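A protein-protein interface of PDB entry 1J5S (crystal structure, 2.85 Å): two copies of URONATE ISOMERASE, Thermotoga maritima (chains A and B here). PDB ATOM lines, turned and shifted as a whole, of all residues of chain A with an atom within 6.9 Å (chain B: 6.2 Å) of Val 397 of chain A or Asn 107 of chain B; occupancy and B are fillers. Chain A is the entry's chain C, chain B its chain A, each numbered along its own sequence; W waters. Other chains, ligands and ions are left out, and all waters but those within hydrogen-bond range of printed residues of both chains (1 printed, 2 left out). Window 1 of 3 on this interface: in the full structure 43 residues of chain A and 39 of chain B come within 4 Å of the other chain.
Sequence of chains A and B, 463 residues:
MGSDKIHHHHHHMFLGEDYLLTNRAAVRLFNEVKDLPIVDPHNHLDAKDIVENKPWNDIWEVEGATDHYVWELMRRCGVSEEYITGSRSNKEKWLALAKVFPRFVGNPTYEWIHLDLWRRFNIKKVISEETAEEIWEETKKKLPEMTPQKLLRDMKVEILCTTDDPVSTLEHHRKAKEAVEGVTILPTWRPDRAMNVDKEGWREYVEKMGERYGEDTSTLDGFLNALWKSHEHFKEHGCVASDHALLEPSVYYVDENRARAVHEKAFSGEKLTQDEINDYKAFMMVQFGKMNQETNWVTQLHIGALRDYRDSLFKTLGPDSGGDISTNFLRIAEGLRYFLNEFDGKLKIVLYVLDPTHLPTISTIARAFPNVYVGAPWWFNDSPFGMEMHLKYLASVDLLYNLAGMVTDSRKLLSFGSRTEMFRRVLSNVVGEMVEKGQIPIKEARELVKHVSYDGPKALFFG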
ATOM      1  N   PRO A 360       3.796 -13.401  39.276  1.00  0.00           N
ATOM      2  CA  PRO A 360       4.617 -12.795  38.220  1.00  0.00           C
ATOM      3  C   PRO A 360       5.958 -13.484  38.025  1.00  0.00           C
ATOM      4  O   PRO A 360       6.370 -13.730  36.887  1.00  0.00           O
ATOM      5  CB  PRO A 360       4.827 -11.378  38.725  1.00  0.00           C
ATOM      6  CG  PRO A 360       3.618 -11.099  39.513  1.00  0.00           C
ATOM      7  CD  PRO A 360       3.290 -12.383  40.212  1.00  0.00           C
ATOM      8  N   SER A 363       5.113 -16.856  36.589  1.00  0.00           N
ATOM      9  CA  SER A 363       4.488 -16.628  35.294  1.00  0.00           C
ATOM     10  C   SER A 363       5.539 -16.277  34.250  1.00  0.00           C
ATOM     11  O   SER A 363       5.567 -16.876  33.169  1.00  0.00           O
ATOM     12  CB  SER A 363       3.424 -15.540  35.402  1.00  0.00           C
ATOM     13  OG  SER A 363       2.439 -15.943  36.342  1.00  0.00           O
ATOM     14  N   THR A 364       6.424 -15.335  34.573  1.00  0.00           N
ATOM     15  CA  THR A 364       7.488 -14.975  33.629  1.00  0.00           C
ATOM     16  C   THR A 364       8.459 -16.134  33.451  1.00  0.00           C
ATOM     17  O   THR A 364       8.949 -16.387  32.350  1.00  0.00           O
ATOM     18  CB  THR A 364       8.250 -13.718  34.061  1.00  0.00           C
ATOM     19  OG1 THR A 364       8.729 -13.863  35.398  1.00  0.00           O
ATOM     20  CG2 THR A 364       7.323 -12.500  34.073  1.00  0.00           C
ATOM     21  N   ARG A 367       6.900 -18.249  31.042  1.00  0.00           N
ATOM     22  CA  ARG A 367       6.907 -17.642  29.719  1.00  0.00           C
ATOM     23  C   ARG A 367       8.218 -17.894  28.986  1.00  0.00           C
ATOM     24  O   ARG A 367       8.290 -17.745  27.770  1.00  0.00           O
ATOM     25  CB  ARG A 367       6.679 -16.129  29.770  1.00  0.00           C
ATOM     26  CG  ARG A 367       6.383 -15.578  28.364  1.00  0.00           C
ATOM     27  CD  ARG A 367       6.543 -14.082  28.132  1.00  0.00           C
ATOM     28  NE  ARG A 367       5.241 -13.421  28.120  1.00  0.00           N
ATOM     29  CZ  ARG A 367       4.905 -12.355  27.384  1.00  0.00           C
ATOM     30  NH1 ARG A 367       5.771 -11.773  26.551  1.00  0.00           N
ATOM     31  NH2 ARG A 367       3.674 -11.861  27.490  1.00  0.00           N
ATOM     32  N   LYS A 392      -6.897 -14.045  35.119  1.00  0.00           N
ATOM     33  CA  LYS A 392      -6.788 -12.851  34.287  1.00  0.00           C
ATOM     34  C   LYS A 392      -5.331 -12.518  34.201  1.00  0.00           C
ATOM     35  O   LYS A 392      -4.785 -12.297  33.139  1.00  0.00           O
ATOM     36  CB  LYS A 392      -7.477 -11.655  34.888  1.00  0.00           C
ATOM     37  CG  LYS A 392      -8.915 -11.800  35.027  1.00  0.00           C
ATOM     38  CD  LYS A 392      -9.453 -10.432  35.258  1.00  0.00           C
ATOM     39  CE  LYS A 392     -10.654 -10.449  36.134  1.00  0.00           C
ATOM     40  NZ  LYS A 392     -10.602  -9.244  36.996  1.00  0.00           N
ATOM     41  N   TYR A 393      -4.696 -12.484  35.354  1.00  0.00           N
ATOM     42  CA  TYR A 393      -3.313 -12.130  35.381  1.00  0.00           C
ATOM     43  C   TYR A 393      -2.480 -13.042  34.490  1.00  0.00           C
ATOM     44  O   TYR A 393      -1.731 -12.563  33.631  1.00  0.00           O
ATOM     45  CB  TYR A 393      -2.741 -12.173  36.784  1.00  0.00           C
ATOM     46  CG  TYR A 393      -1.266 -11.975  36.663  1.00  0.00           C
ATOM     47  CD1 TYR A 393      -0.763 -10.758  36.253  1.00  0.00           C
ATOM     48  CD2 TYR A 393      -0.390 -13.030  36.830  1.00  0.00           C
ATOM     49  CE1 TYR A 393       0.568 -10.576  36.068  1.00  0.00           C
ATOM     50  CE2 TYR A 393       0.944 -12.862  36.657  1.00  0.00           C
ATOM     51  CZ  TYR A 393       1.429 -11.626  36.273  1.00  0.00           C
ATOM     52  OH  TYR A 393       2.790 -11.438  36.093  1.00  0.00           O
ATOM     53  N   LEU A 394      -2.604 -14.352  34.691  1.00  0.00           N
ATOM     54  CA  LEU A 394      -1.795 -15.303  33.939  1.00  0.00           C
ATOM     55  C   LEU A 394      -2.061 -15.204  32.453  1.00  0.00           C
ATOM     56  O   LEU A 394      -1.171 -15.429  31.639  1.00  0.00           O
ATOM     57  CB  LEU A 394      -2.077 -16.726  34.392  1.00  0.00           C
ATOM     58  CG  LEU A 394      -1.252 -17.780  33.657  1.00  0.00           C
ATOM     59  CD1 LEU A 394       0.245 -17.689  33.947  1.00  0.00           C
ATOM     60  CD2 LEU A 394      -1.791 -19.126  34.005  1.00  0.00           C
ATOM     61  N   ALA A 395      -3.295 -14.874  32.105  1.00  0.00           N
ATOM     62  CA  ALA A 395      -3.682 -14.750  30.706  1.00  0.00           C
ATOM     63  C   ALA A 395      -2.980 -13.620  30.020  1.00  0.00           C
ATOM     64  O   ALA A 395      -2.787 -13.666  28.820  1.00  0.00           O
ATOM     65  CB  ALA A 395      -5.168 -14.538  30.574  1.00  0.00           C
ATOM     66  N   SER A 396      -2.607 -12.594  30.767  1.00  0.00           N
ATOM     67  CA  SER A 396      -2.010 -11.414  30.137  1.00  0.00           C
ATOM     68  C   SER A 396      -0.494 -11.502  30.043  1.00  0.00           C
ATOM     69  O   SER A 396       0.147 -10.595  29.539  1.00  0.00           O
ATOM     70  CB  SER A 396      -2.417 -10.135  30.875  1.00  0.00           C
ATOM     71  OG  SER A 396      -1.710 -10.006  32.093  1.00  0.00           O
ATOM     72  N   VAL A 397       0.081 -12.599  30.504  1.00  0.00           N
ATOM     73  CA  VAL A 397       1.527 -12.689  30.544  1.00  0.00           C
ATOM     74  C   VAL A 397       2.082 -13.927  29.869  1.00  0.00           C
ATOM     75  O   VAL A 397       3.113 -13.866  29.219  1.00  0.00           O
ATOM     76  CB  VAL A 397       1.988 -12.635  31.972  1.00  0.00           C
ATOM     77  CG1 VAL A 397       3.493 -12.639  32.022  1.00  0.00           C
ATOM     78  CG2 VAL A 397       1.424 -11.386  32.616  1.00  0.00           C
ATOM     79  N   ASP A 398       1.426 -15.056  30.058  1.00  0.00           N
ATOM     80  CA  ASP A 398       1.794 -16.250  29.333  1.00  0.00           C
ATOM     81  C   ASP A 398       0.509 -16.595  28.609  1.00  0.00           C
ATOM     82  O   ASP A 398      -0.185 -15.679  28.179  1.00  0.00           O
ATOM     83  CB  ASP A 398       2.273 -17.376  30.243  1.00  0.00           C
ATOM     84  CG  ASP A 398       2.799 -18.554  29.453  1.00  0.00           C
ATOM     85  OD1 ASP A 398       2.132 -19.609  29.417  1.00  0.00           O
ATOM     86  OD2 ASP A 398       3.860 -18.502  28.796  1.00  0.00           O
ATOM     87  N   LEU A 399       0.175 -17.880  28.490  1.00  0.00           N
ATOM     88  CA  LEU A 399      -1.052 -18.297  27.818  1.00  0.00           C
ATOM     89  C   LEU A 399      -2.007 -19.025  28.747  1.00  0.00           C
ATOM     90  O   LEU A 399      -1.679 -20.078  29.294  1.00  0.00           O
ATOM     91  CB  LEU A 399      -0.713 -19.212  26.647  1.00  0.00           C
ATOM     92  CG  LEU A 399       0.211 -18.547  25.635  1.00  0.00           C
ATOM     93  CD1 LEU A 399       0.565 -19.494  24.501  1.00  0.00           C
ATOM     94  CD2 LEU A 399      -0.462 -17.298  25.117  1.00  0.00           C
ATOM     95  N   LEU A 400      -3.204 -18.484  28.913  1.00  0.00           N
ATOM     96  CA  LEU A 400      -4.193 -19.149  29.745  1.00  0.00           C
ATOM     97  C   LEU A 400      -4.301 -20.587  29.244  1.00  0.00           C
ATOM     98  O   LEU A 400      -4.434 -21.530  30.009  1.00  0.00           O
ATOM     99  CB  LEU A 400      -5.549 -18.445  29.648  1.00  0.00           C
ATOM    100  CG  LEU A 400      -6.636 -18.783  30.678  1.00  0.00           C
ATOM    101  CD1 LEU A 400      -6.120 -18.928  32.099  1.00  0.00           C
ATOM    102  CD2 LEU A 400      -7.685 -17.695  30.637  1.00  0.00           C
ATOM    103  N   MET A 434     -13.666 -11.368  28.685  1.00  0.00           N
ATOM    104  CA  MET A 434     -12.747 -10.995  27.622  1.00  0.00           C
ATOM    105  C   MET A 434     -13.490 -11.093  26.279  1.00  0.00           C
ATOM    106  O   MET A 434     -13.260 -10.303  25.376  1.00  0.00           O
ATOM    107  CB  MET A 434     -11.492 -11.880  27.658  1.00  0.00           C
ATOM    108  CG  MET A 434     -10.613 -11.677  28.910  1.00  0.00           C
ATOM    109  SD  MET A 434      -9.211 -12.858  29.116  1.00  0.00           S
ATOM    110  CE  MET A 434     -10.087 -14.277  29.176  1.00  0.00           C
ATOM    111  N   GLN A 439     -11.872  -9.017  23.258  1.00  0.00           N
ATOM    112  CA  GLN A 439     -10.482  -9.495  23.195  1.00  0.00           C
ATOM    113  C   GLN A 439     -10.362 -10.916  22.689  1.00  0.00           C
ATOM    114  O   GLN A 439      -9.267 -11.343  22.309  1.00  0.00           O
ATOM    115  CB  GLN A 439      -9.842  -9.493  24.578  1.00  0.00           C
ATOM    116  CG  GLN A 439      -9.834  -8.160  25.243  1.00  0.00           C
ATOM    117  CD  GLN A 439      -9.099  -8.168  26.565  1.00  0.00           C
ATOM    118  OE1 GLN A 439      -9.719  -8.248  27.626  1.00  0.00           O
ATOM    119  NE2 GLN A 439      -7.779  -8.060  26.508  1.00  0.00           N
ATOM    120  N   ILE A 440     -11.452 -11.670  22.731  1.00  0.00           N
ATOM    121  CA  ILE A 440     -11.411 -13.050  22.282  1.00  0.00           C
ATOM    122  C   ILE A 440     -12.668 -13.422  21.520  1.00  0.00           C
ATOM    123  O   ILE A 440     -13.774 -13.293  22.040  1.00  0.00           O
ATOM    124  CB  ILE A 440     -11.240 -14.006  23.486  1.00  0.00           C
ATOM    125  CG1 ILE A 440      -9.933 -13.710  24.220  1.00  0.00           C
ATOM    126  CG2 ILE A 440     -11.281 -15.462  23.007  1.00  0.00           C
ATOM    127  CD1 ILE A 440      -9.779 -14.470  25.506  1.00  0.00           C
ATOM    128  N   LEU B  73       5.880 -16.857  22.620  1.00  0.00           N
ATOM    129  CA  LEU B  73       4.595 -17.534  22.611  1.00  0.00           C
ATOM    130  C   LEU B  73       4.672 -18.716  21.659  1.00  0.00           C
ATOM    131  O   LEU B  73       4.190 -19.801  21.976  1.00  0.00           O
ATOM    132  CB  LEU B  73       3.460 -16.577  22.242  1.00  0.00           C
ATOM    133  CG  LEU B  73       3.410 -15.313  23.116  1.00  0.00           C
ATOM    134  CD1 LEU B  73       2.290 -14.392  22.711  1.00  0.00           C
ATOM    135  CD2 LEU B  73       3.260 -15.684  24.571  1.00  0.00           C
ATOM    136  N   PHE B 104      -3.213 -18.154  21.589  1.00  0.00           N
ATOM    137  CA  PHE B 104      -2.668 -16.929  22.157  1.00  0.00           C
ATOM    138  C   PHE B 104      -3.773 -16.132  22.818  1.00  0.00           C
ATOM    139  O   PHE B 104      -3.543 -15.204  23.589  1.00  0.00           O
ATOM    140  CB  PHE B 104      -2.064 -16.064  21.057  1.00  0.00           C
ATOM    141  CG  PHE B 104      -0.722 -16.523  20.586  1.00  0.00           C
ATOM    142  CD1 PHE B 104      -0.471 -17.862  20.322  1.00  0.00           C
ATOM    143  CD2 PHE B 104       0.284 -15.606  20.381  1.00  0.00           C
ATOM    144  CE1 PHE B 104       0.757 -18.266  19.884  1.00  0.00           C
ATOM    145  CE2 PHE B 104       1.510 -16.010  19.940  1.00  0.00           C
ATOM    146  CZ  PHE B 104       1.750 -17.342  19.693  1.00  0.00           C
ATOM    147  N   VAL B 105      -4.987 -16.488  22.451  1.00  0.00           N
ATOM    148  CA  VAL B 105      -6.178 -15.863  22.959  1.00  0.00           C
ATOM    149  C   VAL B 105      -5.915 -15.431  24.424  1.00  0.00           C
ATOM    150  O   VAL B 105      -5.388 -16.193  25.228  1.00  0.00           O
ATOM    151  CB  VAL B 105      -7.350 -16.881  22.746  1.00  0.00           C
ATOM    152  CG1 VAL B 105      -7.719 -17.626  24.018  1.00  0.00           C
ATOM    153  CG2 VAL B 105      -8.541 -16.213  22.097  1.00  0.00           C
ATOM    154  N   GLY B 106      -6.201 -14.181  24.754  1.00  0.00           N
ATOM    155  CA  GLY B 106      -6.026 -13.707  26.113  1.00  0.00           C
ATOM    156  C   GLY B 106      -4.758 -12.922  26.366  1.00  0.00           C
ATOM    157  O   GLY B 106      -4.670 -12.172  27.339  1.00  0.00           O
ATOM    158  N   ASN B 107      -3.772 -13.085  25.497  1.00  0.00           N
ATOM    159  CA  ASN B 107      -2.475 -12.419  25.663  1.00  0.00           C
ATOM    160  C   ASN B 107      -2.375 -11.222  24.703  1.00  0.00           C
ATOM    161  O   ASN B 107      -2.744 -11.334  23.531  1.00  0.00           O
ATOM    162  CB  ASN B 107      -1.371 -13.444  25.412  1.00  0.00           C
ATOM    163  CG  ASN B 107      -0.001 -12.921  25.729  1.00  0.00           C
ATOM    164  OD1 ASN B 107       0.489 -12.003  25.083  1.00  0.00           O
ATOM    165  ND2 ASN B 107       0.646 -13.528  26.713  1.00  0.00           N
ATOM    166  N   PRO B 108      -1.851 -10.094  25.167  1.00  0.00           N
ATOM    167  CA  PRO B 108      -1.898  -8.857  24.381  1.00  0.00           C
ATOM    168  C   PRO B 108      -1.435  -9.021  22.941  1.00  0.00           C
ATOM    169  O   PRO B 108      -1.965  -8.351  22.051  1.00  0.00           O
ATOM    170  CB  PRO B 108      -0.962  -7.891  25.142  1.00  0.00           C
ATOM    171  CG  PRO B 108      -0.649  -8.510  26.438  1.00  0.00           C
ATOM    172  CD  PRO B 108      -1.125  -9.929  26.431  1.00  0.00           C
ATOM    173  N   THR B 109      -0.472  -9.895  22.692  1.00  0.00           N
ATOM    174  CA  THR B 109      -0.003 -10.037  21.326  1.00  0.00           C
ATOM    175  C   THR B 109      -1.130 -10.485  20.416  1.00  0.00           C
ATOM    176  O   THR B 109      -1.200 -10.071  19.271  1.00  0.00           O
ATOM    177  CB  THR B 109       1.156 -11.009  21.208  1.00  0.00           C
ATOM    178  OG1 THR B 109       2.374 -10.346  21.574  1.00  0.00           O
ATOM    179  CG2 THR B 109       1.370 -11.372  19.752  1.00  0.00           C
ATOM    180  N   TYR B 110      -2.007 -11.341  20.911  1.00  0.00           N
ATOM    181  CA  TYR B 110      -3.118 -11.786  20.088  1.00  0.00           C
ATOM    182  C   TYR B 110      -3.903 -10.575  19.587  1.00  0.00           C
ATOM    183  O   TYR B 110      -4.301 -10.509  18.426  1.00  0.00           O
ATOM    184  CB  TYR B 110      -4.032 -12.713  20.876  1.00  0.00           C
ATOM    185  CG  TYR B 110      -5.155 -13.294  20.053  1.00  0.00           C
ATOM    186  CD1 TYR B 110      -4.967 -14.444  19.306  1.00  0.00           C
ATOM    187  CD2 TYR B 110      -6.400 -12.694  20.030  1.00  0.00           C
ATOM    188  CE1 TYR B 110      -5.991 -14.990  18.576  1.00  0.00           C
ATOM    189  CE2 TYR B 110      -7.434 -13.222  19.290  1.00  0.00           C
ATOM    190  CZ  TYR B 110      -7.232 -14.372  18.562  1.00  0.00           C
ATOM    191  OH  TYR B 110      -8.275 -14.893  17.819  1.00  0.00           O
ATOM    192  N   GLU B 111      -4.085  -9.598  20.460  1.00  0.00           N
ATOM    193  CA  GLU B 111      -4.876  -8.426  20.124  1.00  0.00           C
ATOM    194  C   GLU B 111      -4.089  -7.392  19.309  1.00  0.00           C
ATOM    195  O   GLU B 111      -4.621  -6.801  18.378  1.00  0.00           O
ATOM    196  CB  GLU B 111      -5.459  -7.808  21.408  1.00  0.00           C
ATOM    197  CG  GLU B 111      -6.159  -8.811  22.319  1.00  0.00           C
ATOM    198  CD  GLU B 111      -6.541  -8.208  23.658  1.00  0.00           C
ATOM    199  OE1 GLU B 111      -7.288  -7.214  23.668  1.00  0.00           O
ATOM    200  OE2 GLU B 111      -6.096  -8.716  24.705  1.00  0.00           O
ATOM    201  N   TRP B 112      -2.834  -7.164  19.669  1.00  0.00           N
ATOM    202  CA  TRP B 112      -2.006  -6.227  18.925  1.00  0.00           C
ATOM    203  C   TRP B 112      -1.918  -6.590  17.436  1.00  0.00           C
ATOM    204  O   TRP B 112      -2.191  -5.755  16.564  1.00  0.00           O
ATOM    205  CB  TRP B 112      -0.603  -6.168  19.528  1.00  0.00           C
ATOM    206  CG  TRP B 112      -0.528  -5.354  20.783  1.00  0.00           C
ATOM    207  CD1 TRP B 112      -1.278  -4.263  21.098  1.00  0.00           C
ATOM    208  CD2 TRP B 112       0.358  -5.561  21.886  1.00  0.00           C
ATOM    209  NE1 TRP B 112      -0.918  -3.784  22.333  1.00  0.00           N
ATOM    210  CE2 TRP B 112       0.087  -4.564  22.838  1.00  0.00           C
ATOM    211  CE3 TRP B 112       1.353  -6.495  22.170  1.00  0.00           C
ATOM    212  CZ2 TRP B 112       0.767  -4.479  24.051  1.00  0.00           C
ATOM    213  CZ3 TRP B 112       2.034  -6.401  23.367  1.00  0.00           C
ATOM    214  CH2 TRP B 112       1.734  -5.406  24.294  1.00  0.00           C
ATOM    215  N   PHE B 380       6.123  -7.134  30.678  1.00  0.00           N
ATOM    216  CA  PHE B 380       5.095  -8.146  30.777  1.00  0.00           C
ATOM    217  C   PHE B 380       3.795  -7.492  31.285  1.00  0.00           C
ATOM    218  O   PHE B 380       2.724  -8.086  31.239  1.00  0.00           O
ATOM    219  CB  PHE B 380       5.559  -9.257  31.711  1.00  0.00           C
ATOM    220  CG  PHE B 380       6.900  -9.828  31.354  1.00  0.00           C
ATOM    221  CD1 PHE B 380       8.022  -9.510  32.104  1.00  0.00           C
ATOM    222  CD2 PHE B 380       7.040 -10.686  30.274  1.00  0.00           C
ATOM    223  CE1 PHE B 380       9.263 -10.040  31.784  1.00  0.00           C
ATOM    224  CE2 PHE B 380       8.278 -11.217  29.948  1.00  0.00           C
ATOM    225  CZ  PHE B 380       9.391 -10.891  30.707  1.00  0.00           C
ATOM    226  N   ASN B 381       3.886  -6.254  31.752  1.00  0.00           N
ATOM    227  CA  ASN B 381       2.713  -5.575  32.289  1.00  0.00           C
ATOM    228  C   ASN B 381       1.882  -4.760  31.297  1.00  0.00           C
ATOM    229  O   ASN B 381       0.765  -4.371  31.637  1.00  0.00           O
ATOM    230  CB  ASN B 381       3.109  -4.706  33.473  1.00  0.00           C
ATOM    231  CG  ASN B 381       3.749  -5.507  34.564  1.00  0.00           C
ATOM    232  OD1 ASN B 381       3.132  -6.418  35.109  1.00  0.00           O
ATOM    233  ND2 ASN B 381       4.999  -5.203  34.875  1.00  0.00           N
ATOM    234  N   SER B 383      -0.627  -4.660  29.003  1.00  0.00           N
ATOM    235  CA  SER B 383      -1.680  -5.566  28.656  1.00  0.00           C
ATOM    236  C   SER B 383      -2.888  -4.872  29.246  1.00  0.00           C
ATOM    237  O   SER B 383      -2.783  -4.206  30.267  1.00  0.00           O
ATOM    238  CB  SER B 383      -1.467  -6.893  29.393  1.00  0.00           C
ATOM    239  OG  SER B 383      -1.707  -6.744  30.790  1.00  0.00           O
HETATM  240  O   HOH W   1      -4.631 -18.420  25.869  1.00  0.00           O
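The side-chain amide nitrogen (ND2) of Asn 107 of chain B is in hydrogen-bond range of the backbone carbonyl oxygen (O) of Asp 398 of chain A, 2.7 Å away.
The backbone carbonyl oxygen (O) of Gly 106 of chain B sits close to the backbone carbonyl oxygen (O) of Ala 395 of chain A, at 2.8 Å.
The side-chain amide nitrogen (NE2) of Gln 439 of chain A lies within hydrogen-bond range of the side-chain carboxylate (OE2) of Glu 111 of chain B, 2.6 Å away.
Water W1 bridges O of Val 105 of chain B (2.4 Å) and N of Leu 400 of chain A (3.4 Å).
O of Val 397 of chain A sits at hydrogen-bond distance from NE of Arg 367 of chain A (2.4 Å).
The side-chain amide oxygen (OD1) of Asn 107 of chain B lies close to the backbone NH (N) of Thr 109 of chain B (3.3 Å).
The backbone carbonyl oxygen of Tyr 393 of chain A lies within hydrogen-bond range of the side-chain hydroxyl of Ser 396 of chain A, 3.0 Å away.
The backbone carbonyl oxygen (O) of Pro 360 of chain A is in hydrogen-bond range of the side-chain hydroxyl (OG1) of Thr 364 of chain A (2.8 Å).
O of Met 434 of chain A lies within hydrogen-bond range of N of Ile 440 of chain A (3.5 Å).
The backbone carbonyl oxygen (O) of Met 434 of chain A is in hydrogen-bond range of the backbone NH (N) of Gln 439 of chain A, 2.8 Å away.
Among the printed residues, pairs that only touch across the chains: Thr 364 of chain A with Phe 380 of chain B, Arg 367 of chain A with Asn 107 of chain B, Arg 367 of chain A with Phe 380 of chain B, Ala 395 of chain A with Asn 107 of chain B, Ser 396 of chain A with Gly 106 of chain B, Ser 396 of chain A with Pro 108 of chain B, Ser 396 of chain A with Phe 380 of chain B, Ser 396 of chain A with Ser 383 of chain B, Val 397 of chain A with Asn 107 of chain B, Val 397 of chain A with Phe 380 of chain B, Leu 399 of chain A with Phe 104 of chain B, Leu 399 of chain A with Asn 107 of chain B, Gln 439 of chain A with Tyr 110 of chain B, Ile 440 of chain A with Val 105 of chain B and Ile 440 of chain A with Gly 106 of chain B.
Of the printed residues of chain B, Val 397 of chain A touches Asn 107 (3.5 Å) and Phe 380 (3.8 Å).
Asn 107 of chain B touches just these residues of chain A: Arg 367 (3.5 Å), Ala 395 (3.4 Å), Val 397 (3.5 Å), Asp 398 (2.7 Å) and Leu 399 (3.97 Å).
Of chain A, only Ala 395 (2.8 Å), Ser 396 (3.9 Å) and Ile 440 (3.7 Å) come within 4 Å of Gly 106 of chain B.
Printed residues of chain B within 4 Å of Arg 367 of chain A: Asn 107 (3.5 Å) and Phe 380 (3.8 Å).
Of the printed residues of chain A, Ser 383 of chain B touches Ser 396 (3.5 Å).
Printed residues of chain A within 4 Å of Val 105 of chain B: Ile 440 (3.0 Å).
Leu 73 of chain B touches none of the printed residues of chain A.
The nearest residue of chain A that does not touch Asn 107 of chain B is Ser 396 of chain A (4.1 Å).
Printed residues of chain B that touch a printed residue of chain A: Phe 104, Val 105, Gly 106, Asn 107, Pro 108, Tyr 110, Glu 111, Phe 380 and Ser 383.
Hydrophobic or aromatic side chains of chain B within 4 Å of the printed part of chain A: Val 105, Pro 108, Tyr 110 and Phe 380.
Along chain B the printed residues that touch a printed residue of chain A span positions 104 to 383.
Hydrophobic or aromatic side chains of chain A that line the printed part of chain B: Val 397, Leu 399 and Ile 440.
Along chain A the printed residues that touch a printed residue of chain B span positions 364 to 440.
No position is printed for both chains.
Of the 18 pairs that touch across the chains among the printed residues, none has its exchanged pair printed and touching as well.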
